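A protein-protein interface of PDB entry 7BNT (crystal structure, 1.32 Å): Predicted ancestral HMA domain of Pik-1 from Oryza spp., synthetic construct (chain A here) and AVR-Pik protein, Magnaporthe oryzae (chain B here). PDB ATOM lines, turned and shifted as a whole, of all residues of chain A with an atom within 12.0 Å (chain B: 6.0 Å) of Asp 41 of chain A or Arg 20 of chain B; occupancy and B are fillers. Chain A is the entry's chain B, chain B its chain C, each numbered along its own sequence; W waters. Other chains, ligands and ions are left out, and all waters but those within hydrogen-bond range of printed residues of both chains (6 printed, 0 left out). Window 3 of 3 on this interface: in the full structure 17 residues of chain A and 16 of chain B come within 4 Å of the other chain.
The guanidinium group (NH1) of Arg 20 of chain A lies within hydrogen-bond range of the backbone carbonyl oxygen (O) of Arg 43 of chain A (2.9 Å).
N of Val 39 of chain A lies within hydrogen-bond range of O of Lys 45 of chain A, at 2.8 Å.
NZ of Lys 45 of chain A lies within salt-bridge range of OD1 of Asp 44 of chain A.
The guanidinium group of Arg 45 of chain B is in salt-bridge range of the side-chain carboxylate of Glu 19 of chain B (2.8 Å).
The backbone carbonyl oxygen (O) of Arg 20 of chain B lies within hydrogen-bond range of the guanidinium group (NH1) of Arg 45 of chain B, at 2.9 Å.
Among the printed residues, pairs that only touch across the chains: Gly 40 of chain A with Asp 47 of chain B, Asp 41 of chain A with Asn 23 of chain B, Asp 41 of chain A with Gln 46 of chain B, Asp 41 of chain A with Ala 48 of chain B and Arg 43 of chain A with Asn 23 of chain B.
Among the printed residues, Asp or Glu carboxylates within 4 Å of a Lys or Arg side-chain nitrogen of the other chain: Asp 41 of chain A with Arg 20 of chain B (3.9 Å), Asp 41 of chain A with Arg 45 of chain B (2.8 Å) and Lys 45 of chain A with Asp 47 of chain B (3.1 Å).
Water W3 bridges the side-chain amide nitrogen of Asn 23 of chain B and the backbone carbonyl oxygen of Asp 41 of chain A.
Water W5 bridges the side-chain carboxylate of Asp 41 of chain A (2.6 Å) and the backbone carbonyl oxygen of Arg 45 of chain B (3.3 Å).
Water W1 lies within hydrogen-bond range of O of Asn 23 of chain B, O of Ala 48 of chain B and N of Gly 40 of chain A.
Water W6 lies within hydrogen-bond range of the side-chain carboxylate of Asp 41 of chain A (2.7 Å), the backbone NH of Asn 23 of chain B (2.8 Å) and the backbone carbonyl oxygen of Ala 48 of chain B (3.3 Å).
Water W4 lies within hydrogen-bond range of NH2 of Arg 20 of chain B (2.9 Å) and O of Asp 41 of chain A (2.9 Å).
Water W2 bridges O of Ala 48 of chain B (3.1 Å) and N of Gly 40 of chain A (3.5 Å).
O of Gly 40 of chain A is in hydrogen-bond range of ND2 of Asn 23 of chain B, at 2.9 Å.
The side-chain carboxylate of Asp 41 of chain A lies within salt-bridge range of the guanidinium group of Arg 20 of chain B, 3.9 Å away.
The side-chain carboxylate of Asp 41 of chain A is in salt-bridge range of the guanidinium group of Arg 45 of chain B (2.8 Å).
N of Asp 41 of chain A is in hydrogen-bond range of OD1 of Asp 47 of chain B, 2.9 Å away.
The side-chain amino group of Lys 45 of chain A lies within salt-bridge range of the side-chain carboxylate of Asp 47 of chain B.
Of chain B, only Arg 20, Asn 23, Arg 45, Gln 46, Asp 47 and Ala 48 come within 4 Å of Asp 41 of chain A.
Of chain A, only Asp 41 comes within 4 Å of Arg 20 of chain B.
No residue of chain A comes within 4 Å of Glu 19 of chain B.
No residue of chain A comes within 4 Å of Asp 21 of chain B.
Pro 22 of chain B touches none of the printed residues of chain A.
Asn 23 of chain B touches just these residues of chain A: Gly 40, Asp 41 and Arg 43.
Arg 45 of chain B touches one residue of chain A.
Ala 48 of chain B touches just one residue of chain A: Asp 41 (3.7 Å).
Printed residues of chain B within 4 Å of Lys 45 of chain A: Asp 47 (3.1 Å).
Printed residues of chain A within 4 Å of Gln 46 of chain B: Asp 41 (3.95 Å).
Of the printed residues of chain B, Arg 43 of chain A touches Asn 23.
Leu 42 of chain A touches none of the printed residues of chain B.
Val 39 of chain A touches none of the printed residues of chain B.
The nearest residue of chain B that does not touch Asp 41 of chain A is Pro 22 of chain B (4.8 Å).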
ATOM      1  N   VAL A   9      17.626  17.426 -12.967  1.00  0.00           N
ATOM      2  CA  VAL A   9      18.700  17.934 -13.849  1.00  0.00           C
ATOM      3  C   VAL A   9      19.045  19.347 -13.391  1.00  0.00           C
ATOM      4  O   VAL A   9      18.144  20.188 -13.275  1.00  0.00           O
ATOM      5  CB  VAL A   9      18.286  17.929 -15.322  1.00  0.00           C
ATOM      6  CG1 VAL A   9      19.422  18.436 -16.182  1.00  0.00           C
ATOM      7  CG2 VAL A   9      17.867  16.534 -15.754  1.00  0.00           C
ATOM      8  N   ILE A  10      20.326  19.574 -13.154  1.00  0.00           N
ATOM      9  CA  ILE A  10      20.862  20.870 -12.695  1.00  0.00           C
ATOM     10  C   ILE A  10      21.946  21.327 -13.672  1.00  0.00           C
ATOM     11  O   ILE A  10      22.883  20.575 -13.948  1.00  0.00           O
ATOM     12  CB  ILE A  10      21.382  20.793 -11.243  1.00  0.00           C
ATOM     13  CG1 ILE A  10      20.245  20.464 -10.274  1.00  0.00           C
ATOM     14  CG2 ILE A  10      22.060  22.096 -10.865  1.00  0.00           C
ATOM     15  CD1 ILE A  10      20.712  20.086  -8.875  1.00  0.00           C
ATOM     16  N   LYS A  11      21.806  22.540 -14.183  1.00  0.00           N
ATOM     17  CA  LYS A  11      22.849  23.174 -15.016  1.00  0.00           C
ATOM     18  C   LYS A  11      23.969  23.655 -14.092  1.00  0.00           C
ATOM     19  O   LYS A  11      23.676  24.282 -13.047  1.00  0.00           O
ATOM     20  CB  LYS A  11      22.287  24.347 -15.817  1.00  0.00           C
ATOM     21  CG  LYS A  11      23.294  24.984 -16.781  1.00  0.00           C
ATOM     22  CD  LYS A  11      22.613  25.882 -17.808  1.00  0.00           C
ATOM     23  CE  LYS A  11      23.550  26.595 -18.754  1.00  0.00           C
ATOM     24  NZ  LYS A  11      22.803  27.443 -19.720  1.00  0.00           N
ATOM     25  N   VAL A  12      25.188  23.289 -14.437  1.00  0.00           N
ATOM     26  CA  VAL A  12      26.347  23.575 -13.561  1.00  0.00           C
ATOM     27  C   VAL A  12      27.307  24.479 -14.291  1.00  0.00           C
ATOM     28  O   VAL A  12      27.339  24.505 -15.513  1.00  0.00           O
ATOM     29  CB  VAL A  12      27.053  22.302 -13.081  1.00  0.00           C
ATOM     30  CG1 VAL A  12      26.124  21.499 -12.183  1.00  0.00           C
ATOM     31  CG2 VAL A  12      27.579  21.469 -14.239  1.00  0.00           C
ATOM     32  N   MET A  14      30.468  25.976 -16.051  1.00  0.00           N
ATOM     33  CA  MET A  14      31.400  25.459 -17.057  1.00  0.00           C
ATOM     34  C   MET A  14      32.663  26.315 -17.080  1.00  0.00           C
ATOM     35  O   MET A  14      33.302  26.383 -18.130  1.00  0.00           O
ATOM     36  CB  MET A  14      30.684  25.459 -18.406  1.00  0.00           C
ATOM     37  CG  MET A  14      29.494  24.513 -18.407  1.00  0.00           C
ATOM     38  SD  MET A  14      30.009  22.780 -18.367  1.00  0.00           S
ATOM     39  CE  MET A  14      30.380  22.540 -20.109  1.00  0.00           C
ATOM     40  N   ARG A  20      33.549  21.632 -13.439  1.00  0.00           N
ATOM     41  CA  ARG A  20      32.450  20.706 -13.761  1.00  0.00           C
ATOM     42  C   ARG A  20      32.642  19.412 -12.955  1.00  0.00           C
ATOM     43  O   ARG A  20      31.659  18.897 -12.389  1.00  0.00           O
ATOM     44  CB  ARG A  20      32.389  20.486 -15.268  1.00  0.00           C
ATOM     45  CG  ARG A  20      31.242  19.589 -15.688  1.00  0.00           C
ATOM     46  CD  ARG A  20      31.119  19.494 -17.196  1.00  0.00           C
ATOM     47  NE  ARG A  20      32.293  18.848 -17.754  1.00  0.00           N
ATOM     48  CZ  ARG A  20      32.477  18.557 -19.034  1.00  0.00           C
ATOM     49  NH1 ARG A  20      31.565  18.876 -19.930  1.00  0.00           N
ATOM     50  NH2 ARG A  20      33.595  17.963 -19.415  1.00  0.00           N
ATOM     51  N   ALA A  37      25.103  11.760 -14.052  1.00  0.00           N
ATOM     52  CA  ALA A  37      25.636  11.769 -15.429  1.00  0.00           C
ATOM     53  C   ALA A  37      25.664  13.188 -15.967  1.00  0.00           C
ATOM     54  O   ALA A  37      24.768  13.986 -15.686  1.00  0.00           O
ATOM     55  CB  ALA A  37      24.805  10.883 -16.333  1.00  0.00           C
ATOM     56  N   LEU A  38      26.679  13.456 -16.774  1.00  0.00           N
ATOM     57  CA  LEU A  38      26.720  14.695 -17.567  1.00  0.00           C
ATOM     58  C   LEU A  38      25.795  14.540 -18.775  1.00  0.00           C
ATOM     59  O   LEU A  38      25.955  13.597 -19.552  1.00  0.00           O
ATOM     60  CB  LEU A  38      28.130  14.990 -18.034  1.00  0.00           C
ATOM     61  CG  LEU A  38      29.057  15.478 -16.955  1.00  0.00           C
ATOM     62  CD1 LEU A  38      30.462  15.599 -17.532  1.00  0.00           C
ATOM     63  CD2 LEU A  38      28.577  16.817 -16.420  1.00  0.00           C
ATOM     64  N   VAL A  39      24.859  15.443 -18.907  1.00  0.00           N
ATOM     65  CA  VAL A  39      23.834  15.425 -19.965  1.00  0.00           C
ATOM     66  C   VAL A  39      23.763  16.841 -20.544  1.00  0.00           C
ATOM     67  O   VAL A  39      24.555  17.721 -20.196  1.00  0.00           O
ATOM     68  CB  VAL A  39      22.467  14.926 -19.430  1.00  0.00           C
ATOM     69  CG1 VAL A  39      22.569  13.507 -18.933  1.00  0.00           C
ATOM     70  CG2 VAL A  39      21.849  15.841 -18.384  1.00  0.00           C
ATOM     71  N   GLY A  40      22.857  17.001 -21.471  1.00  0.00           N
ATOM     72  CA  GLY A  40      22.680  18.245 -22.213  1.00  0.00           C
ATOM     73  C   GLY A  40      23.461  18.211 -23.505  1.00  0.00           C
ATOM     74  O   GLY A  40      24.480  17.500 -23.620  1.00  0.00           O
ATOM     75  N   ASP A  41      22.999  18.964 -24.493  1.00  0.00           N
ATOM     76  CA  ASP A  41      23.728  19.051 -25.788  1.00  0.00           C
ATOM     77  C   ASP A  41      25.176  19.527 -25.586  1.00  0.00           C
ATOM     78  O   ASP A  41      26.013  19.135 -26.365  1.00  0.00           O
ATOM     79  CB  ASP A  41      22.953  19.908 -26.779  1.00  0.00           C
ATOM     80  CG  ASP A  41      21.751  19.247 -27.424  1.00  0.00           C
ATOM     81  OD1 ASP A  41      21.569  18.026 -27.254  1.00  0.00           O
ATOM     82  OD2 ASP A  41      21.026  19.943 -28.155  1.00  0.00           O
ATOM     83  N   LEU A  42      25.435  20.358 -24.589  1.00  0.00           N
ATOM     84  CA  LEU A  42      26.789  20.861 -24.292  1.00  0.00           C
ATOM     85  C   LEU A  42      27.405  20.191 -23.055  1.00  0.00           C
ATOM     86  O   LEU A  42      28.427  20.679 -22.588  1.00  0.00           O
ATOM     87  CB  LEU A  42      26.711  22.377 -24.096  1.00  0.00           C
ATOM     88  CG  LEU A  42      26.208  23.146 -25.311  1.00  0.00           C
ATOM     89  CD1 LEU A  42      26.028  24.620 -24.980  1.00  0.00           C
ATOM     90  CD2 LEU A  42      27.157  22.966 -26.486  1.00  0.00           C
ATOM     91  N   ARG A  43      26.848  19.113 -22.535  1.00  0.00           N
ATOM     92  CA  ARG A  43      27.426  18.397 -21.376  1.00  0.00           C
ATOM     93  C   ARG A  43      27.694  19.407 -20.255  1.00  0.00           C
ATOM     94  O   ARG A  43      28.756  19.351 -19.585  1.00  0.00           O
ATOM     95  CB  ARG A  43      28.649  17.607 -21.837  1.00  0.00           C
ATOM     96  CG  ARG A  43      28.265  16.557 -22.868  1.00  0.00           C
ATOM     97  CD  ARG A  43      29.413  15.699 -23.325  1.00  0.00           C
ATOM     98  NE  ARG A  43      29.412  14.559 -22.433  1.00  0.00           N
ATOM     99  CZ  ARG A  43      30.354  14.283 -21.545  1.00  0.00           C
ATOM    100  NH1 ARG A  43      31.440  15.043 -21.448  1.00  0.00           N
ATOM    101  NH2 ARG A  43      30.229  13.204 -20.795  1.00  0.00           N
ATOM    102  N   ASP A  44      26.703  20.244 -19.994  1.00  0.00           N
ATOM    103  CA  ASP A  44      26.747  21.334 -18.988  1.00  0.00           C
ATOM    104  C   ASP A  44      25.700  21.101 -17.898  1.00  0.00           C
ATOM    105  O   ASP A  44      25.419  22.028 -17.107  1.00  0.00           O
ATOM    106  CB  ASP A  44      26.526  22.682 -19.677  1.00  0.00           C
ATOM    107  CG  ASP A  44      25.239  22.839 -20.462  1.00  0.00           C
ATOM    108  OD1 ASP A  44      24.548  21.830 -20.669  1.00  0.00           O
ATOM    109  OD2 ASP A  44      24.947  24.009 -20.870  1.00  0.00           O
ATOM    110  N   LYS A  45      25.109  19.923 -17.863  1.00  0.00           N
ATOM    111  CA  LYS A  45      24.069  19.614 -16.876  1.00  0.00           C
ATOM    112  C   LYS A  45      24.394  18.290 -16.229  1.00  0.00           C
ATOM    113  O   LYS A  45      24.926  17.406 -16.887  1.00  0.00           O
ATOM    114  CB  LYS A  45      22.701  19.590 -17.541  1.00  0.00           C
ATOM    115  CG  LYS A  45      22.304  20.918 -18.162  1.00  0.00           C
ATOM    116  CD  LYS A  45      21.257  20.784 -19.191  1.00  0.00           C
ATOM    117  CE  LYS A  45      20.976  22.097 -19.867  1.00  0.00           C
ATOM    118  NZ  LYS A  45      21.666  22.202 -21.154  1.00  0.00           N
ATOM    119  N   ILE A  46      24.036  18.199 -14.959  1.00  0.00           N
ATOM    120  CA  ILE A  46      24.161  16.954 -14.186  1.00  0.00           C
ATOM    121  C   ILE A  46      22.761  16.425 -13.964  1.00  0.00           C
ATOM    122  O   ILE A  46      21.901  17.132 -13.429  1.00  0.00           O
ATOM    123  CB  ILE A  46      24.906  17.159 -12.861  1.00  0.00           C
ATOM    124  CG1 ILE A  46      26.301  17.757 -13.075  1.00  0.00           C
ATOM    125  CG2 ILE A  46      24.967  15.846 -12.079  1.00  0.00           C
ATOM    126  CD1 ILE A  46      26.985  18.133 -11.793  1.00  0.00           C
ATOM    127  N   GLU A  47      22.553  15.210 -14.438  1.00  0.00           N
ATOM    128  CA  GLU A  47      21.319  14.453 -14.155  1.00  0.00           C
ATOM    129  C   GLU A  47      21.592  13.538 -12.971  1.00  0.00           C
ATOM    130  O   GLU A  47      22.538  12.739 -13.023  1.00  0.00           O
ATOM    131  CB  GLU A  47      20.955  13.657 -15.382  1.00  0.00           C
ATOM    132  CG  GLU A  47      19.609  13.019 -15.349  1.00  0.00           C
ATOM    133  CD  GLU A  47      19.364  12.436 -16.746  1.00  0.00           C
ATOM    134  OE1 GLU A  47      19.796  11.304 -17.012  1.00  0.00           O
ATOM    135  OE2 GLU A  47      18.825  13.160 -17.624  1.00  0.00           O
ATOM    136  N   LEU A  72      16.775  22.583 -13.712  1.00  0.00           N
ATOM    137  CA  LEU A  72      16.122  22.656 -15.028  1.00  0.00           C
ATOM    138  C   LEU A  72      15.070  21.581 -15.240  1.00  0.00           C
ATOM    139  O   LEU A  72      14.293  21.735 -16.190  1.00  0.00           O
ATOM    140  CB  LEU A  72      17.166  22.587 -16.145  1.00  0.00           C
ATOM    141  CG  LEU A  72      18.163  23.739 -16.211  1.00  0.00           C
ATOM    142  CD1 LEU A  72      19.053  23.523 -17.414  1.00  0.00           C
ATOM    143  CD2 LEU A  72      17.495  25.097 -16.307  1.00  0.00           C
ATOM    144  N   GLN A  73      15.083  20.489 -14.476  1.00  0.00           N
ATOM    145  CA  GLN A  73      14.077  19.441 -14.712  1.00  0.00           C
ATOM    146  C   GLN A  73      13.863  18.676 -13.417  1.00  0.00           C
ATOM    147  O   GLN A  73      14.847  18.403 -12.722  1.00  0.00           O
ATOM    148  CB  GLN A  73      14.550  18.472 -15.798  1.00  0.00           C
ATOM    149  CG  GLN A  73      13.469  17.525 -16.291  1.00  0.00           C
ATOM    150  CD  GLN A  73      13.993  16.427 -17.179  1.00  0.00           C
ATOM    151  OE1 GLN A  73      14.683  16.669 -18.164  1.00  0.00           O
ATOM    152  NE2 GLN A  73      13.607  15.218 -16.846  1.00  0.00           N
ATOM    153  N   ARG B  18      15.982  13.720 -38.584  1.00  0.00           N
ATOM    154  CA  ARG B  18      17.378  14.056 -38.941  1.00  0.00           C
ATOM    155  C   ARG B  18      18.140  14.567 -37.727  1.00  0.00           C
ATOM    156  O   ARG B  18      19.312  14.882 -37.857  1.00  0.00           O
ATOM    157  CB  ARG B  18      17.402  15.088 -40.066  1.00  0.00           C
ATOM    158  CG  ARG B  18      16.931  14.485 -41.385  1.00  0.00           C
ATOM    159  CD  ARG B  18      16.905  15.454 -42.551  1.00  0.00           C
ATOM    160  NE  ARG B  18      18.203  16.082 -42.751  1.00  0.00           N
ATOM    161  CZ  ARG B  18      18.394  17.297 -43.262  1.00  0.00           C
ATOM    162  NH1 ARG B  18      19.622  17.769 -43.377  1.00  0.00           N
ATOM    163  NH2 ARG B  18      17.368  18.047 -43.636  1.00  0.00           N
ATOM    164  N   GLU B  19      17.514  14.628 -36.563  1.00  0.00           N
ATOM    165  CA  GLU B  19      18.189  15.148 -35.351  1.00  0.00           C
ATOM    166  C   GLU B  19      19.116  14.073 -34.794  1.00  0.00           C
ATOM    167  O   GLU B  19      18.715  12.915 -34.659  1.00  0.00           O
ATOM    168  CB  GLU B  19      17.165  15.563 -34.293  1.00  0.00           C
ATOM    169  CG  GLU B  19      16.555  16.916 -34.557  1.00  0.00           C
ATOM    170  CD  GLU B  19      17.525  18.085 -34.486  1.00  0.00           C
ATOM    171  OE1 GLU B  19      18.666  17.890 -33.987  1.00  0.00           O
ATOM    172  OE2 GLU B  19      17.123  19.190 -34.870  1.00  0.00           O
ATOM    173  N   ARG B  20      20.313  14.484 -34.417  1.00  0.00           N
ATOM    174  CA  ARG B  20      21.249  13.562 -33.739  1.00  0.00           C
ATOM    175  C   ARG B  20      20.674  13.164 -32.380  1.00  0.00           C
ATOM    176  O   ARG B  20      20.037  13.962 -31.683  1.00  0.00           O
ATOM    177  CB  ARG B  20      22.633  14.174 -33.587  1.00  0.00           C
ATOM    178  CG  ARG B  20      22.718  15.340 -32.631  1.00  0.00           C
ATOM    179  CD  ARG B  20      24.002  16.115 -32.831  1.00  0.00           C
ATOM    180  NE  ARG B  20      24.170  17.133 -31.811  1.00  0.00           N
ATOM    181  CZ  ARG B  20      23.568  18.318 -31.809  1.00  0.00           C
ATOM    182  NH1 ARG B  20      22.743  18.637 -32.789  1.00  0.00           N
ATOM    183  NH2 ARG B  20      23.783  19.171 -30.819  1.00  0.00           N
ATOM    184  N   ASP B  21      20.937  11.938 -31.994  1.00  0.00           N
ATOM    185  CA  ASP B  21      20.439  11.464 -30.690  1.00  0.00           C
ATOM    186  C   ASP B  21      21.010  12.365 -29.598  1.00  0.00           C
ATOM    187  O   ASP B  21      22.156  12.805 -29.626  1.00  0.00           O
ATOM    188  CB  ASP B  21      20.857  10.025 -30.411  1.00  0.00           C
ATOM    189  CG  ASP B  21      20.169   8.966 -31.259  1.00  0.00           C
ATOM    190  OD1 ASP B  21      19.218   9.318 -31.988  1.00  0.00           O
ATOM    191  OD2 ASP B  21      20.581   7.776 -31.148  1.00  0.00           O
ATOM    192  N   PRO B  22      20.215  12.626 -28.553  1.00  0.00           N
ATOM    193  CA  PRO B  22      20.734  13.332 -27.400  1.00  0.00           C
ATOM    194  C   PRO B  22      21.855  12.570 -26.687  1.00  0.00           C
ATOM    195  O   PRO B  22      21.918  11.374 -26.762  1.00  0.00           O
ATOM    196  CB  PRO B  22      19.545  13.394 -26.436  1.00  0.00           C
ATOM    197  CG  PRO B  22      18.341  12.985 -27.242  1.00  0.00           C
ATOM    198  CD  PRO B  22      18.823  12.200 -28.422  1.00  0.00           C
ATOM    199  N   ASN B  23      22.596  13.305 -25.877  1.00  0.00           N
ATOM    200  CA  ASN B  23      23.414  12.722 -24.800  1.00  0.00           C
ATOM    201  C   ASN B  23      22.484  12.136 -23.745  1.00  0.00           C
ATOM    202  O   ASN B  23      21.502  12.755 -23.354  1.00  0.00           O
ATOM    203  CB  ASN B  23      24.338  13.758 -24.175  1.00  0.00           C
ATOM    204  CG  ASN B  23      25.444  14.163 -25.116  1.00  0.00           C
ATOM    205  OD1 ASN B  23      26.021  13.329 -25.808  1.00  0.00           O
ATOM    206  ND2 ASN B  23      25.751  15.450 -25.144  1.00  0.00           N
ATOM    207  N   PHE B  38      13.348  16.917 -27.602  1.00  0.00           N
ATOM    208  CA  PHE B  38      14.200  17.963 -28.218  1.00  0.00           C
ATOM    209  C   PHE B  38      13.513  19.301 -28.004  1.00  0.00           C
ATOM    210  O   PHE B  38      12.292  19.450 -28.271  1.00  0.00           O
ATOM    211  CB  PHE B  38      14.313  17.697 -29.721  1.00  0.00           C
ATOM    212  CG  PHE B  38      14.886  16.347 -30.050  1.00  0.00           C
ATOM    213  CD1 PHE B  38      14.053  15.226 -30.117  1.00  0.00           C
ATOM    214  CD2 PHE B  38      16.234  16.194 -30.329  1.00  0.00           C
ATOM    215  CE1 PHE B  38      14.572  13.976 -30.414  1.00  0.00           C
ATOM    216  CE2 PHE B  38      16.746  14.935 -30.592  1.00  0.00           C
ATOM    217  CZ  PHE B  38      15.915  13.835 -30.672  1.00  0.00           C
ATOM    218  N   ARG B  45      17.465  24.024 -32.457  1.00  0.00           N
ATOM    219  CA  ARG B  45      17.659  23.101 -31.319  1.00  0.00           C
ATOM    220  C   ARG B  45      18.468  23.760 -30.204  1.00  0.00           C
ATOM    221  O   ARG B  45      19.547  24.296 -30.461  1.00  0.00           O
ATOM    222  CB  ARG B  45      18.304  21.807 -31.800  1.00  0.00           C
ATOM    223  CG  ARG B  45      18.610  20.850 -30.653  1.00  0.00           C
ATOM    224  CD  ARG B  45      19.061  19.525 -31.231  1.00  0.00           C
ATOM    225  NE  ARG B  45      19.662  18.648 -30.258  1.00  0.00           N
ATOM    226  CZ  ARG B  45      19.978  17.372 -30.495  1.00  0.00           C
ATOM    227  NH1 ARG B  45      19.658  16.794 -31.643  1.00  0.00           N
ATOM    228  NH2 ARG B  45      20.608  16.684 -29.563  1.00  0.00           N
ATOM    229  N   GLN B  46      17.953  23.692 -28.982  1.00  0.00           N
ATOM    230  CA  GLN B  46      18.609  24.253 -27.777  1.00  0.00           C
ATOM    231  C   GLN B  46      19.110  23.143 -26.853  1.00  0.00           C
ATOM    232  O   GLN B  46      20.123  23.338 -26.186  1.00  0.00           O
ATOM    233  CB  GLN B  46      17.597  25.107 -27.013  1.00  0.00           C
ATOM    234  CG  GLN B  46      17.052  26.248 -27.840  1.00  0.00           C
ATOM    235  CD  GLN B  46      18.143  27.188 -28.278  1.00  0.00           C
ATOM    236  OE1 GLN B  46      18.960  27.662 -27.475  1.00  0.00           O
ATOM    237  NE2 GLN B  46      18.218  27.439 -29.568  1.00  0.00           N
ATOM    238  N   ASP B  47      18.390  22.032 -26.751  1.00  0.00           N
ATOM    239  CA  ASP B  47      18.798  20.952 -25.825  1.00  0.00           C
ATOM    240  C   ASP B  47      17.984  19.714 -26.183  1.00  0.00           C
ATOM    241  O   ASP B  47      17.033  19.794 -26.990  1.00  0.00           O
ATOM    242  CB  ASP B  47      18.546  21.356 -24.373  1.00  0.00           C
ATOM    243  CG  ASP B  47      19.359  20.587 -23.357  1.00  0.00           C
ATOM    244  OD1 ASP B  47      20.336  19.907 -23.763  1.00  0.00           O
ATOM    245  OD2 ASP B  47      19.061  20.773 -22.147  1.00  0.00           O
ATOM    246  N   ALA B  48      18.339  18.598 -25.578  1.00  0.00           N
ATOM    247  CA  ALA B  48      17.650  17.327 -25.842  1.00  0.00           C
ATOM    248  C   ALA B  48      17.982  16.351 -24.730  1.00  0.00           C
ATOM    249  O   ALA B  48      18.968  16.574 -24.016  1.00  0.00           O
ATOM    250  CB  ALA B  48      18.085  16.777 -27.178  1.00  0.00           C
ATOM    251  N   GLY B  49      17.175  15.306 -24.600  1.00  0.00           N
ATOM    252  CA  GLY B  49      17.429  14.299 -23.568  1.00  0.00           C
ATOM    253  C   GLY B  49      16.477  13.151 -23.715  1.00  0.00           C
ATOM    254  O   GLY B  49      15.816  13.013 -24.741  1.00  0.00           O
HETATM  255  O   HOH W   1      21.060  15.314 -22.902  1.00  0.00           O
HETATM  256  O   HOH W   2      19.436  17.438 -21.055  1.00  0.00           O
HETATM  257  O   HOH W   3      27.628  16.849 -25.987  1.00  0.00           O
HETATM  258  O   HOH W   4      26.062  19.760 -29.176  1.00  0.00           O
HETATM  259  O   HOH W   5      21.839  22.175 -29.255  1.00  0.00           O
HETATM  260  O   HOH W   6      21.857  16.033 -25.529  1.00  0.00           O
